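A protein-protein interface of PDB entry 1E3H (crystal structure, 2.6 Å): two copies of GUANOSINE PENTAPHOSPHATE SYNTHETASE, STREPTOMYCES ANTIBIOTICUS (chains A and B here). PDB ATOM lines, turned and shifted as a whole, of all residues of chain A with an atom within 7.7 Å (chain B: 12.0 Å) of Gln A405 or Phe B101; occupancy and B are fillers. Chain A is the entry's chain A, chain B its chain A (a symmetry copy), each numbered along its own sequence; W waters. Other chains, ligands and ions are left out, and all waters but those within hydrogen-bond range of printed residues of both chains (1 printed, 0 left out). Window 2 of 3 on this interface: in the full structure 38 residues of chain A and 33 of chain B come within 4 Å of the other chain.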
ATOM      1  N   GLY A  99      -9.331 -14.116  23.296  1.00  0.00           N
ATOM      2  CA  GLY A  99      -9.124 -15.552  23.275  1.00  0.00           C
ATOM      3  C   GLY A  99      -7.865 -16.063  23.955  1.00  0.00           C
ATOM      4  O   GLY A  99      -7.732 -17.273  24.171  1.00  0.00           O
ATOM      5  N   SER A 100      -6.943 -15.164  24.294  1.00  0.00           N
ATOM      6  CA  SER A 100      -5.701 -15.576  24.944  1.00  0.00           C
ATOM      7  C   SER A 100      -5.969 -16.250  26.287  1.00  0.00           C
ATOM      8  O   SER A 100      -7.049 -16.100  26.866  1.00  0.00           O
ATOM      9  CB  SER A 100      -4.761 -14.375  25.136  1.00  0.00           C
ATOM     10  OG  SER A 100      -5.352 -13.369  25.939  1.00  0.00           O
ATOM     11  N   ARG A 107       0.224  -7.930  24.121  1.00  0.00           N
ATOM     12  CA  ARG A 107       1.120  -7.345  23.124  1.00  0.00           C
ATOM     13  C   ARG A 107       0.375  -7.035  21.830  1.00  0.00           C
ATOM     14  O   ARG A 107      -0.214  -7.922  21.210  1.00  0.00           O
ATOM     15  CB  ARG A 107       2.318  -8.267  22.855  1.00  0.00           C
ATOM     16  CG  ARG A 107       1.976  -9.719  22.561  1.00  0.00           C
ATOM     17  CD  ARG A 107       3.256 -10.535  22.442  1.00  0.00           C
ATOM     18  NE  ARG A 107       3.001 -11.966  22.315  1.00  0.00           N
ATOM     19  CZ  ARG A 107       3.957 -12.888  22.216  1.00  0.00           C
ATOM     20  NH1 ARG A 107       5.234 -12.527  22.233  1.00  0.00           N
ATOM     21  NH2 ARG A 107       3.637 -14.173  22.102  1.00  0.00           N
ATOM     22  N   LEU A 400      -1.063 -26.391   4.942  1.00  0.00           N
ATOM     23  CA  LEU A 400      -1.917 -25.299   5.381  1.00  0.00           C
ATOM     24  C   LEU A 400      -2.199 -25.265   6.880  1.00  0.00           C
ATOM     25  O   LEU A 400      -2.426 -24.192   7.444  1.00  0.00           O
ATOM     26  CB  LEU A 400      -3.214 -25.317   4.581  1.00  0.00           C
ATOM     27  CG  LEU A 400      -2.965 -24.904   3.126  1.00  0.00           C
ATOM     28  CD1 LEU A 400      -4.185 -25.204   2.285  1.00  0.00           C
ATOM     29  CD2 LEU A 400      -2.616 -23.414   3.068  1.00  0.00           C
ATOM     30  N   ARG A 401      -2.165 -26.419   7.538  1.00  0.00           N
ATOM     31  CA  ARG A 401      -2.413 -26.445   8.975  1.00  0.00           C
ATOM     32  C   ARG A 401      -1.363 -25.615   9.728  1.00  0.00           C
ATOM     33  O   ARG A 401      -1.505 -25.367  10.920  1.00  0.00           O
ATOM     34  CB  ARG A 401      -2.414 -27.885   9.496  1.00  0.00           C
ATOM     35  CG  ARG A 401      -1.048 -28.523   9.565  1.00  0.00           C
ATOM     36  CD  ARG A 401      -1.131 -30.008   9.873  1.00  0.00           C
ATOM     37  NE  ARG A 401       0.202 -30.600   9.983  1.00  0.00           N
ATOM     38  CZ  ARG A 401       0.461 -31.904   9.891  1.00  0.00           C
ATOM     39  NH1 ARG A 401      -0.520 -32.772   9.664  1.00  0.00           N
ATOM     40  NH2 ARG A 401       1.710 -32.342  10.011  1.00  0.00           N
ATOM     41  N   MET A 402      -0.312 -25.189   9.028  1.00  0.00           N
ATOM     42  CA  MET A 402       0.747 -24.375   9.634  1.00  0.00           C
ATOM     43  C   MET A 402       0.544 -22.884   9.401  1.00  0.00           C
ATOM     44  O   MET A 402       1.341 -22.072   9.865  1.00  0.00           O
ATOM     45  CB  MET A 402       2.132 -24.763   9.092  1.00  0.00           C
ATOM     46  CG  MET A 402       2.642 -26.115   9.563  1.00  0.00           C
ATOM     47  SD  MET A 402       2.412 -26.345  11.480  1.00  0.00           S
ATOM     48  CE  MET A 402       3.367 -24.770  12.124  1.00  0.00           C
ATOM     49  N   GLU A 403      -0.505 -22.514   8.672  1.00  0.00           N
ATOM     50  CA  GLU A 403      -0.756 -21.103   8.424  1.00  0.00           C
ATOM     51  C   GLU A 403      -1.067 -20.431   9.762  1.00  0.00           C
ATOM     52  O   GLU A 403      -1.581 -21.066  10.683  1.00  0.00           O
ATOM     53  CB  GLU A 403      -1.918 -20.926   7.442  1.00  0.00           C
ATOM     54  CG  GLU A 403      -3.294 -21.008   8.061  1.00  0.00           C
ATOM     55  CD  GLU A 403      -4.386 -21.274   7.031  1.00  0.00           C
ATOM     56  OE1 GLU A 403      -4.310 -20.703   5.917  1.00  0.00           O
ATOM     57  OE2 GLU A 403      -5.322 -22.047   7.344  1.00  0.00           O
ATOM     58  N   GLN A 404      -0.745 -19.150   9.872  1.00  0.00           N
ATOM     59  CA  GLN A 404      -0.977 -18.418  11.105  1.00  0.00           C
ATOM     60  C   GLN A 404      -2.453 -18.171  11.411  1.00  0.00           C
ATOM     61  O   GLN A 404      -3.242 -17.888  10.509  1.00  0.00           O
ATOM     62  CB  GLN A 404      -0.231 -17.086  11.054  1.00  0.00           C
ATOM     63  CG  GLN A 404      -0.459 -16.203  12.269  1.00  0.00           C
ATOM     64  CD  GLN A 404       0.376 -14.939  12.235  1.00  0.00           C
ATOM     65  OE1 GLN A 404       0.877 -14.539  11.183  1.00  0.00           O
ATOM     66  NE2 GLN A 404       0.517 -14.293  13.389  1.00  0.00           N
ATOM     67  N   GLN A 405      -2.814 -18.293  12.688  1.00  0.00           N
ATOM     68  CA  GLN A 405      -4.184 -18.057  13.152  1.00  0.00           C
ATOM     69  C   GLN A 405      -4.198 -16.707  13.882  1.00  0.00           C
ATOM     70  O   GLN A 405      -3.346 -16.443  14.733  1.00  0.00           O
ATOM     71  CB  GLN A 405      -4.634 -19.174  14.106  1.00  0.00           C
ATOM     72  CG  GLN A 405      -4.883 -20.536  13.451  1.00  0.00           C
ATOM     73  CD  GLN A 405      -6.053 -20.522  12.466  1.00  0.00           C
ATOM     74  OE1 GLN A 405      -5.939 -20.009  11.350  1.00  0.00           O
ATOM     75  NE2 GLN A 405      -7.189 -21.077  12.884  1.00  0.00           N
ATOM     76  N   LEU A 406      -5.162 -15.858  13.547  1.00  0.00           N
ATOM     77  CA  LEU A 406      -5.262 -14.525  14.129  1.00  0.00           C
ATOM     78  C   LEU A 406      -6.597 -14.233  14.807  1.00  0.00           C
ATOM     79  O   LEU A 406      -7.658 -14.582  14.294  1.00  0.00           O
ATOM     80  CB  LEU A 406      -5.024 -13.479  13.040  1.00  0.00           C
ATOM     81  CG  LEU A 406      -3.687 -13.520  12.302  1.00  0.00           C
ATOM     82  CD1 LEU A 406      -3.744 -12.608  11.097  1.00  0.00           C
ATOM     83  CD2 LEU A 406      -2.569 -13.092  13.237  1.00  0.00           C
ATOM     84  N   ASP A 407      -6.532 -13.570  15.956  1.00  0.00           N
ATOM     85  CA  ASP A 407      -7.725 -13.214  16.713  1.00  0.00           C
ATOM     86  C   ASP A 407      -7.615 -11.762  17.178  1.00  0.00           C
ATOM     87  O   ASP A 407      -7.348 -11.483  18.340  1.00  0.00           O
ATOM     88  CB  ASP A 407      -7.876 -14.138  17.923  1.00  0.00           C
ATOM     89  CG  ASP A 407      -9.241 -14.017  18.574  1.00  0.00           C
ATOM     90  OD1 ASP A 407     -10.082 -13.255  18.049  1.00  0.00           O
ATOM     91  OD2 ASP A 407      -9.476 -14.685  19.602  1.00  0.00           O
ATOM     92  N   THR A 408      -7.828 -10.837  16.255  1.00  0.00           N
ATOM     93  CA  THR A 408      -7.720  -9.419  16.556  1.00  0.00           C
ATOM     94  C   THR A 408      -9.002  -8.705  16.128  1.00  0.00           C
ATOM     95  O   THR A 408     -10.019  -9.345  15.868  1.00  0.00           O
ATOM     96  CB  THR A 408      -6.514  -8.814  15.797  1.00  0.00           C
ATOM     97  OG1 THR A 408      -6.798  -8.788  14.392  1.00  0.00           O
ATOM     98  CG2 THR A 408      -5.269  -9.667  16.008  1.00  0.00           C
ATOM     99  N   VAL A 412      -9.712 -10.770   9.254  1.00  0.00           N
ATOM    100  CA  VAL A 412      -8.696 -11.757   8.888  1.00  0.00           C
ATOM    101  C   VAL A 412      -8.441 -12.698  10.063  1.00  0.00           C
ATOM    102  O   VAL A 412      -8.052 -12.257  11.141  1.00  0.00           O
ATOM    103  CB  VAL A 412      -7.363 -11.063   8.514  1.00  0.00           C
ATOM    104  CG1 VAL A 412      -6.295 -12.102   8.199  1.00  0.00           C
ATOM    105  CG2 VAL A 412      -7.576 -10.137   7.336  1.00  0.00           C
ATOM    106  N   THR A 413      -8.643 -13.992   9.840  1.00  0.00           N
ATOM    107  CA  THR A 413      -8.463 -14.993  10.886  1.00  0.00           C
ATOM    108  C   THR A 413      -7.329 -15.967  10.588  1.00  0.00           C
ATOM    109  O   THR A 413      -6.893 -16.710  11.463  1.00  0.00           O
ATOM    110  CB  THR A 413      -9.762 -15.807  11.082  1.00  0.00           C
ATOM    111  OG1 THR A 413     -10.089 -16.492   9.866  1.00  0.00           O
ATOM    112  CG2 THR A 413     -10.909 -14.890  11.440  1.00  0.00           C
ATOM    113  N   ARG A 414      -6.869 -15.986   9.344  1.00  0.00           N
ATOM    114  CA  ARG A 414      -5.784 -16.876   8.959  1.00  0.00           C
ATOM    115  C   ARG A 414      -4.876 -16.153   7.974  1.00  0.00           C
ATOM    116  O   ARG A 414      -5.301 -15.227   7.287  1.00  0.00           O
ATOM    117  CB  ARG A 414      -6.336 -18.151   8.316  1.00  0.00           C
ATOM    118  CG  ARG A 414      -7.056 -17.909   7.005  1.00  0.00           C
ATOM    119  CD  ARG A 414      -8.511 -18.335   7.094  1.00  0.00           C
ATOM    120  NE  ARG A 414      -8.774 -19.572   6.363  1.00  0.00           N
ATOM    121  CZ  ARG A 414      -8.763 -19.672   5.037  1.00  0.00           C
ATOM    122  NH1 ARG A 414      -8.504 -18.606   4.287  1.00  0.00           N
ATOM    123  NH2 ARG A 414      -9.017 -20.839   4.460  1.00  0.00           N
ATOM    124  N   LYS A 415      -3.624 -16.577   7.905  1.00  0.00           N
ATOM    125  CA  LYS A 415      -2.678 -15.945   7.007  1.00  0.00           C
ATOM    126  C   LYS A 415      -1.830 -17.028   6.347  1.00  0.00           C
ATOM    127  O   LYS A 415      -0.971 -17.647   6.982  1.00  0.00           O
ATOM    128  CB  LYS A 415      -1.824 -14.985   7.815  1.00  0.00           C
ATOM    129  CG  LYS A 415      -1.307 -13.792   7.068  1.00  0.00           C
ATOM    130  CD  LYS A 415      -0.674 -12.842   8.064  1.00  0.00           C
ATOM    131  CE  LYS A 415       0.078 -11.729   7.380  1.00  0.00           C
ATOM    132  NZ  LYS A 415       0.749 -10.875   8.381  1.00  0.00           N
ATOM    133  N   MET A 418       3.220 -15.583   5.081  1.00  0.00           N
ATOM    134  CA  MET A 418       3.806 -14.848   6.199  1.00  0.00           C
ATOM    135  C   MET A 418       5.191 -14.317   5.873  1.00  0.00           C
ATOM    136  O   MET A 418       6.045 -15.062   5.397  1.00  0.00           O
ATOM    137  CB  MET A 418       3.912 -15.761   7.419  1.00  0.00           C
ATOM    138  CG  MET A 418       2.577 -16.261   7.955  1.00  0.00           C
ATOM    139  SD  MET A 418       2.711 -18.016   8.807  1.00  0.00           S
ATOM    140  CE  MET A 418       2.280 -19.081   7.242  1.00  0.00           C
ATOM    141  N   ARG A 459      -5.025 -20.315  -2.933  1.00  0.00           N
ATOM    142  CA  ARG A 459      -4.964 -21.382  -1.946  1.00  0.00           C
ATOM    143  C   ARG A 459      -5.204 -22.736  -2.607  1.00  0.00           C
ATOM    144  O   ARG A 459      -4.598 -23.738  -2.240  1.00  0.00           O
ATOM    145  CB  ARG A 459      -6.031 -21.133  -0.888  1.00  0.00           C
ATOM    146  CG  ARG A 459      -5.956 -22.033   0.306  1.00  0.00           C
ATOM    147  CD  ARG A 459      -7.194 -21.856   1.161  1.00  0.00           C
ATOM    148  NE  ARG A 459      -7.007 -22.419   2.492  1.00  0.00           N
ATOM    149  CZ  ARG A 459      -6.316 -21.823   3.456  1.00  0.00           C
ATOM    150  NH1 ARG A 459      -5.752 -20.640   3.235  1.00  0.00           N
ATOM    151  NH2 ARG A 459      -6.178 -22.419   4.633  1.00  0.00           N
ATOM    152  N   MET B  91      13.997 -21.649  12.363  1.00  0.00           N
ATOM    153  CA  MET B  91      13.230 -22.852  12.054  1.00  0.00           C
ATOM    154  C   MET B  91      13.279 -23.221  10.579  1.00  0.00           C
ATOM    155  O   MET B  91      13.090 -24.389  10.228  1.00  0.00           O
ATOM    156  CB  MET B  91      11.763 -22.712  12.502  1.00  0.00           C
ATOM    157  CG  MET B  91      11.554 -22.743  14.024  1.00  0.00           C
ATOM    158  SD  MET B  91      12.586 -24.136  14.928  1.00  0.00           S
ATOM    159  CE  MET B  91      11.571 -25.674  14.340  1.00  0.00           C
ATOM    160  N   ILE B  97       7.823 -24.220   9.587  1.00  0.00           N
ATOM    161  CA  ILE B  97       7.304 -22.945  10.045  1.00  0.00           C
ATOM    162  C   ILE B  97       7.178 -23.019  11.564  1.00  0.00           C
ATOM    163  O   ILE B  97       6.676 -24.001  12.103  1.00  0.00           O
ATOM    164  CB  ILE B  97       5.931 -22.671   9.392  1.00  0.00           C
ATOM    165  CG1 ILE B  97       6.112 -22.570   7.874  1.00  0.00           C
ATOM    166  CG2 ILE B  97       5.301 -21.408   9.967  1.00  0.00           C
ATOM    167  CD1 ILE B  97       4.857 -22.217   7.106  1.00  0.00           C
ATOM    168  N   PRO B  98       7.654 -21.992  12.278  1.00  0.00           N
ATOM    169  CA  PRO B  98       7.553 -22.029  13.744  1.00  0.00           C
ATOM    170  C   PRO B  98       6.141 -22.392  14.193  1.00  0.00           C
ATOM    171  O   PRO B  98       5.148 -21.849  13.678  1.00  0.00           O
ATOM    172  CB  PRO B  98       7.944 -20.615  14.156  1.00  0.00           C
ATOM    173  CG  PRO B  98       8.906 -20.205  13.076  1.00  0.00           C
ATOM    174  CD  PRO B  98       8.227 -20.714  11.818  1.00  0.00           C
ATOM    175  N   GLY B  99       6.056 -23.307  15.152  1.00  0.00           N
ATOM    176  CA  GLY B  99       4.763 -23.745  15.643  1.00  0.00           C
ATOM    177  C   GLY B  99       4.059 -22.815  16.615  1.00  0.00           C
ATOM    178  O   GLY B  99       2.871 -23.008  16.901  1.00  0.00           O
ATOM    179  N   SER B 100       4.768 -21.810  17.126  1.00  0.00           N
ATOM    180  CA  SER B 100       4.167 -20.876  18.074  1.00  0.00           C
ATOM    181  C   SER B 100       2.993 -20.124  17.451  1.00  0.00           C
ATOM    182  O   SER B 100       2.857 -20.067  16.226  1.00  0.00           O
ATOM    183  CB  SER B 100       5.213 -19.877  18.596  1.00  0.00           C
ATOM    184  OG  SER B 100       5.781 -19.116  17.546  1.00  0.00           O
ATOM    185  N   PHE B 101       2.146 -19.565  18.314  1.00  0.00           N
ATOM    186  CA  PHE B 101       0.962 -18.807  17.904  1.00  0.00           C
ATOM    187  C   PHE B 101       1.315 -17.701  16.905  1.00  0.00           C
ATOM    188  O   PHE B 101       0.572 -17.453  15.950  1.00  0.00           O
ATOM    189  CB  PHE B 101       0.296 -18.193  19.146  1.00  0.00           C
ATOM    190  CG  PHE B 101      -0.999 -17.469  18.866  1.00  0.00           C
ATOM    191  CD1 PHE B 101      -2.113 -18.156  18.382  1.00  0.00           C
ATOM    192  CD2 PHE B 101      -1.117 -16.101  19.134  1.00  0.00           C
ATOM    193  CE1 PHE B 101      -3.336 -17.491  18.173  1.00  0.00           C
ATOM    194  CE2 PHE B 101      -2.331 -15.425  18.930  1.00  0.00           C
ATOM    195  CZ  PHE B 101      -3.442 -16.122  18.449  1.00  0.00           C
ATOM    196  N   PHE B 102       2.451 -17.046  17.126  1.00  0.00           N
ATOM    197  CA  PHE B 102       2.881 -15.966  16.246  1.00  0.00           C
ATOM    198  C   PHE B 102       3.666 -16.413  15.013  1.00  0.00           C
ATOM    199  O   PHE B 102       4.125 -15.583  14.232  1.00  0.00           O
ATOM    200  CB  PHE B 102       3.676 -14.933  17.050  1.00  0.00           C
ATOM    201  CG  PHE B 102       2.804 -13.955  17.794  1.00  0.00           C
ATOM    202  CD1 PHE B 102       1.844 -14.405  18.701  1.00  0.00           C
ATOM    203  CD2 PHE B 102       2.911 -12.585  17.557  1.00  0.00           C
ATOM    204  CE1 PHE B 102       1.000 -13.509  19.360  1.00  0.00           C
ATOM    205  CE2 PHE B 102       2.073 -11.676  18.209  1.00  0.00           C
ATOM    206  CZ  PHE B 102       1.113 -12.143  19.114  1.00  0.00           C
ATOM    207  N   ARG B 103       3.802 -17.724  14.843  1.00  0.00           N
ATOM    208  CA  ARG B 103       4.502 -18.307  13.698  1.00  0.00           C
ATOM    209  C   ARG B 103       5.859 -17.670  13.420  1.00  0.00           C
ATOM    210  O   ARG B 103       6.291 -17.569  12.272  1.00  0.00           O
ATOM    211  CB  ARG B 103       3.616 -18.219  12.448  1.00  0.00           C
ATOM    212  CG  ARG B 103       2.337 -19.043  12.539  1.00  0.00           C
ATOM    213  CD  ARG B 103       2.643 -20.531  12.521  1.00  0.00           C
ATOM    214  NE  ARG B 103       1.435 -21.348  12.477  1.00  0.00           N
ATOM    215  CZ  ARG B 103       0.782 -21.796  13.549  1.00  0.00           C
ATOM    216  NH1 ARG B 103       1.218 -21.516  14.773  1.00  0.00           N
ATOM    217  NH2 ARG B 103      -0.313 -22.530  13.395  1.00  0.00           N
ATOM    218  N   ARG B 104       6.524 -17.236  14.482  1.00  0.00           N
ATOM    219  CA  ARG B 104       7.841 -16.624  14.374  1.00  0.00           C
ATOM    220  C   ARG B 104       8.600 -17.107  15.597  1.00  0.00           C
ATOM    221  O   ARG B 104       8.025 -17.201  16.677  1.00  0.00           O
ATOM    222  CB  ARG B 104       7.717 -15.096  14.381  1.00  0.00           C
ATOM    223  CG  ARG B 104       9.006 -14.350  14.053  1.00  0.00           C
ATOM    224  CD  ARG B 104       8.718 -12.905  13.647  1.00  0.00           C
ATOM    225  NE  ARG B 104       9.925 -12.172  13.259  1.00  0.00           N
ATOM    226  CZ  ARG B 104       9.921 -10.968  12.687  1.00  0.00           C
ATOM    227  NH1 ARG B 104       8.773 -10.353  12.428  1.00  0.00           N
ATOM    228  NH2 ARG B 104      11.067 -10.374  12.375  1.00  0.00           N
ATOM    229  N   GLU B 105       9.874 -17.448  15.436  1.00  0.00           N
ATOM    230  CA  GLU B 105      10.639 -17.914  16.582  1.00  0.00           C
ATOM    231  C   GLU B 105      10.932 -16.745  17.534  1.00  0.00           C
ATOM    232  O   GLU B 105      11.278 -15.645  17.095  1.00  0.00           O
ATOM    233  CB  GLU B 105      11.932 -18.642  16.136  1.00  0.00           C
ATOM    234  CG  GLU B 105      12.820 -17.967  15.096  1.00  0.00           C
ATOM    235  CD  GLU B 105      12.304 -18.085  13.665  1.00  0.00           C
ATOM    236  OE1 GLU B 105      12.634 -19.067  12.959  1.00  0.00           O
ATOM    237  OE2 GLU B 105      11.561 -17.181  13.248  1.00  0.00           O
ATOM    238  N   GLY B 106      10.753 -16.988  18.834  1.00  0.00           N
ATOM    239  CA  GLY B 106      10.964 -15.947  19.827  1.00  0.00           C
ATOM    240  C   GLY B 106      12.048 -16.199  20.859  1.00  0.00           C
ATOM    241  O   GLY B 106      13.219 -16.344  20.507  1.00  0.00           O
ATOM    242  N   ARG B 107      11.665 -16.236  22.136  1.00  0.00           N
ATOM    243  CA  ARG B 107      12.636 -16.458  23.207  1.00  0.00           C
ATOM    244  C   ARG B 107      13.425 -17.742  22.976  1.00  0.00           C
ATOM    245  O   ARG B 107      12.852 -18.828  22.871  1.00  0.00           O
ATOM    246  CB  ARG B 107      11.945 -16.482  24.578  1.00  0.00           C
ATOM    247  CG  ARG B 107      10.731 -17.392  24.684  1.00  0.00           C
ATOM    248  CD  ARG B 107      10.078 -17.219  26.048  1.00  0.00           C
ATOM    249  NE  ARG B 107       8.817 -17.945  26.165  1.00  0.00           N
ATOM    250  CZ  ARG B 107       8.048 -17.935  27.252  1.00  0.00           C
ATOM    251  NH1 ARG B 107       8.412 -17.232  28.318  1.00  0.00           N
ATOM    252  NH2 ARG B 107       6.914 -18.627  27.274  1.00  0.00           N
ATOM    253  N   ASP B 407       9.654 -27.944  20.402  1.00  0.00           N
ATOM    254  CA  ASP B 407       9.630 -27.715  18.963  1.00  0.00           C
ATOM    255  C   ASP B 407      10.767 -26.767  18.582  1.00  0.00           C
ATOM    256  O   ASP B 407      10.553 -25.591  18.313  1.00  0.00           O
ATOM    257  CB  ASP B 407       8.287 -27.112  18.549  1.00  0.00           C
ATOM    258  CG  ASP B 407       8.086 -27.131  17.045  1.00  0.00           C
ATOM    259  OD1 ASP B 407       8.969 -27.661  16.336  1.00  0.00           O
ATOM    260  OD2 ASP B 407       7.048 -26.622  16.574  1.00  0.00           O
HETATM  261  O   HOH W   1      -1.056 -19.232  14.757  1.00  0.00           O
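The side-chain carboxylate of Glu A403 is in salt-bridge range of the guanidinium group of Arg A459, at 2.8 Å.
The side-chain sulfur of Met A418 is in hydrogen-bond range of the backbone NH of Gln A404, at 3.8 Å.
O of Gly B99 is in hydrogen-bond range of NH1 of Arg B103, at 3.1 Å.
O of Gln A404 lies within hydrogen-bond range of N of Lys A415, at 2.9 Å.
The side-chain amide oxygen of Gln A405 sits close to the backbone carbonyl oxygen of Thr A413, 3.4 Å away.
The backbone carbonyl oxygen (O) of Ser B100 lies within hydrogen-bond range of the guanidinium group (NH1) of Arg B103 (2.6 Å).
The guanidinium group (NE) of Arg B103 lies within hydrogen-bond range of the backbone carbonyl oxygen (O) of Met A402, 2.7 Å away.
The backbone carbonyl oxygen (O) of Glu A403 is in hydrogen-bond range of the guanidinium group (NH2) of Arg B103, 3.3 Å away.
Printed residues of chain B that touch a printed residue of chain A: Ile B97, Pro B98, Gly B99, Phe B101, Phe B102 and Arg B103.
Hydrophobic or aromatic side chains of chain B that line the printed part of chain A: Phe B101 and Phe B102.
Among the printed residues, 11 pairs touch across the chains.
Among the printed residues, no Asp or Glu carboxylate lies within 4 Å of a Lys or Arg side-chain nitrogen of the other chain.
Water W1 lies within hydrogen-bond range of O of Phe B101 (2.7 Å), N of Gln A405 (2.9 Å) and NH1 of Arg B103 (3.2 Å).
No residue of chain B comes within 4 Å of Gly A99.
Of the printed residues of chain B, Arg A107 touches Phe B102.
Leu A400 touches none of the printed residues of chain B.
Of the printed residues of chain B, Met A402 touches Ile B97, Pro B98, Gly B99 and Arg B103.
Glu A403 touches one residue of chain B.
Of chain B, only Phe B101 (3.6 Å) comes within 4 Å of Gln A405.
No residue of chain B comes within 4 Å of Leu A406.
No residue of chain B comes within 4 Å of Asp A407.
Thr A408 touches none of the printed residues of chain B.
No residue of chain B comes within 4 Å of Thr A413.
No residue of chain B comes within 4 Å of Arg A414.
Printed residues of chain A within 4 Å of Gly B99: Met A402.
Printed residues of chain A within 4 Å of Phe B101: Gln A405.
Among the printed residues, merely in contact across the chains: Arg A107 with Phe B102, Arg A401 with Arg B103, Met A402 with Ile B97, Met A402 with Pro B98, Met A402 with Gly B99, Gln A404 with Phe B102, Gln A404 with Arg B103, Gln A405 with Phe B101 and Met A418 with Arg B103.
4 positions are printed for both chains.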
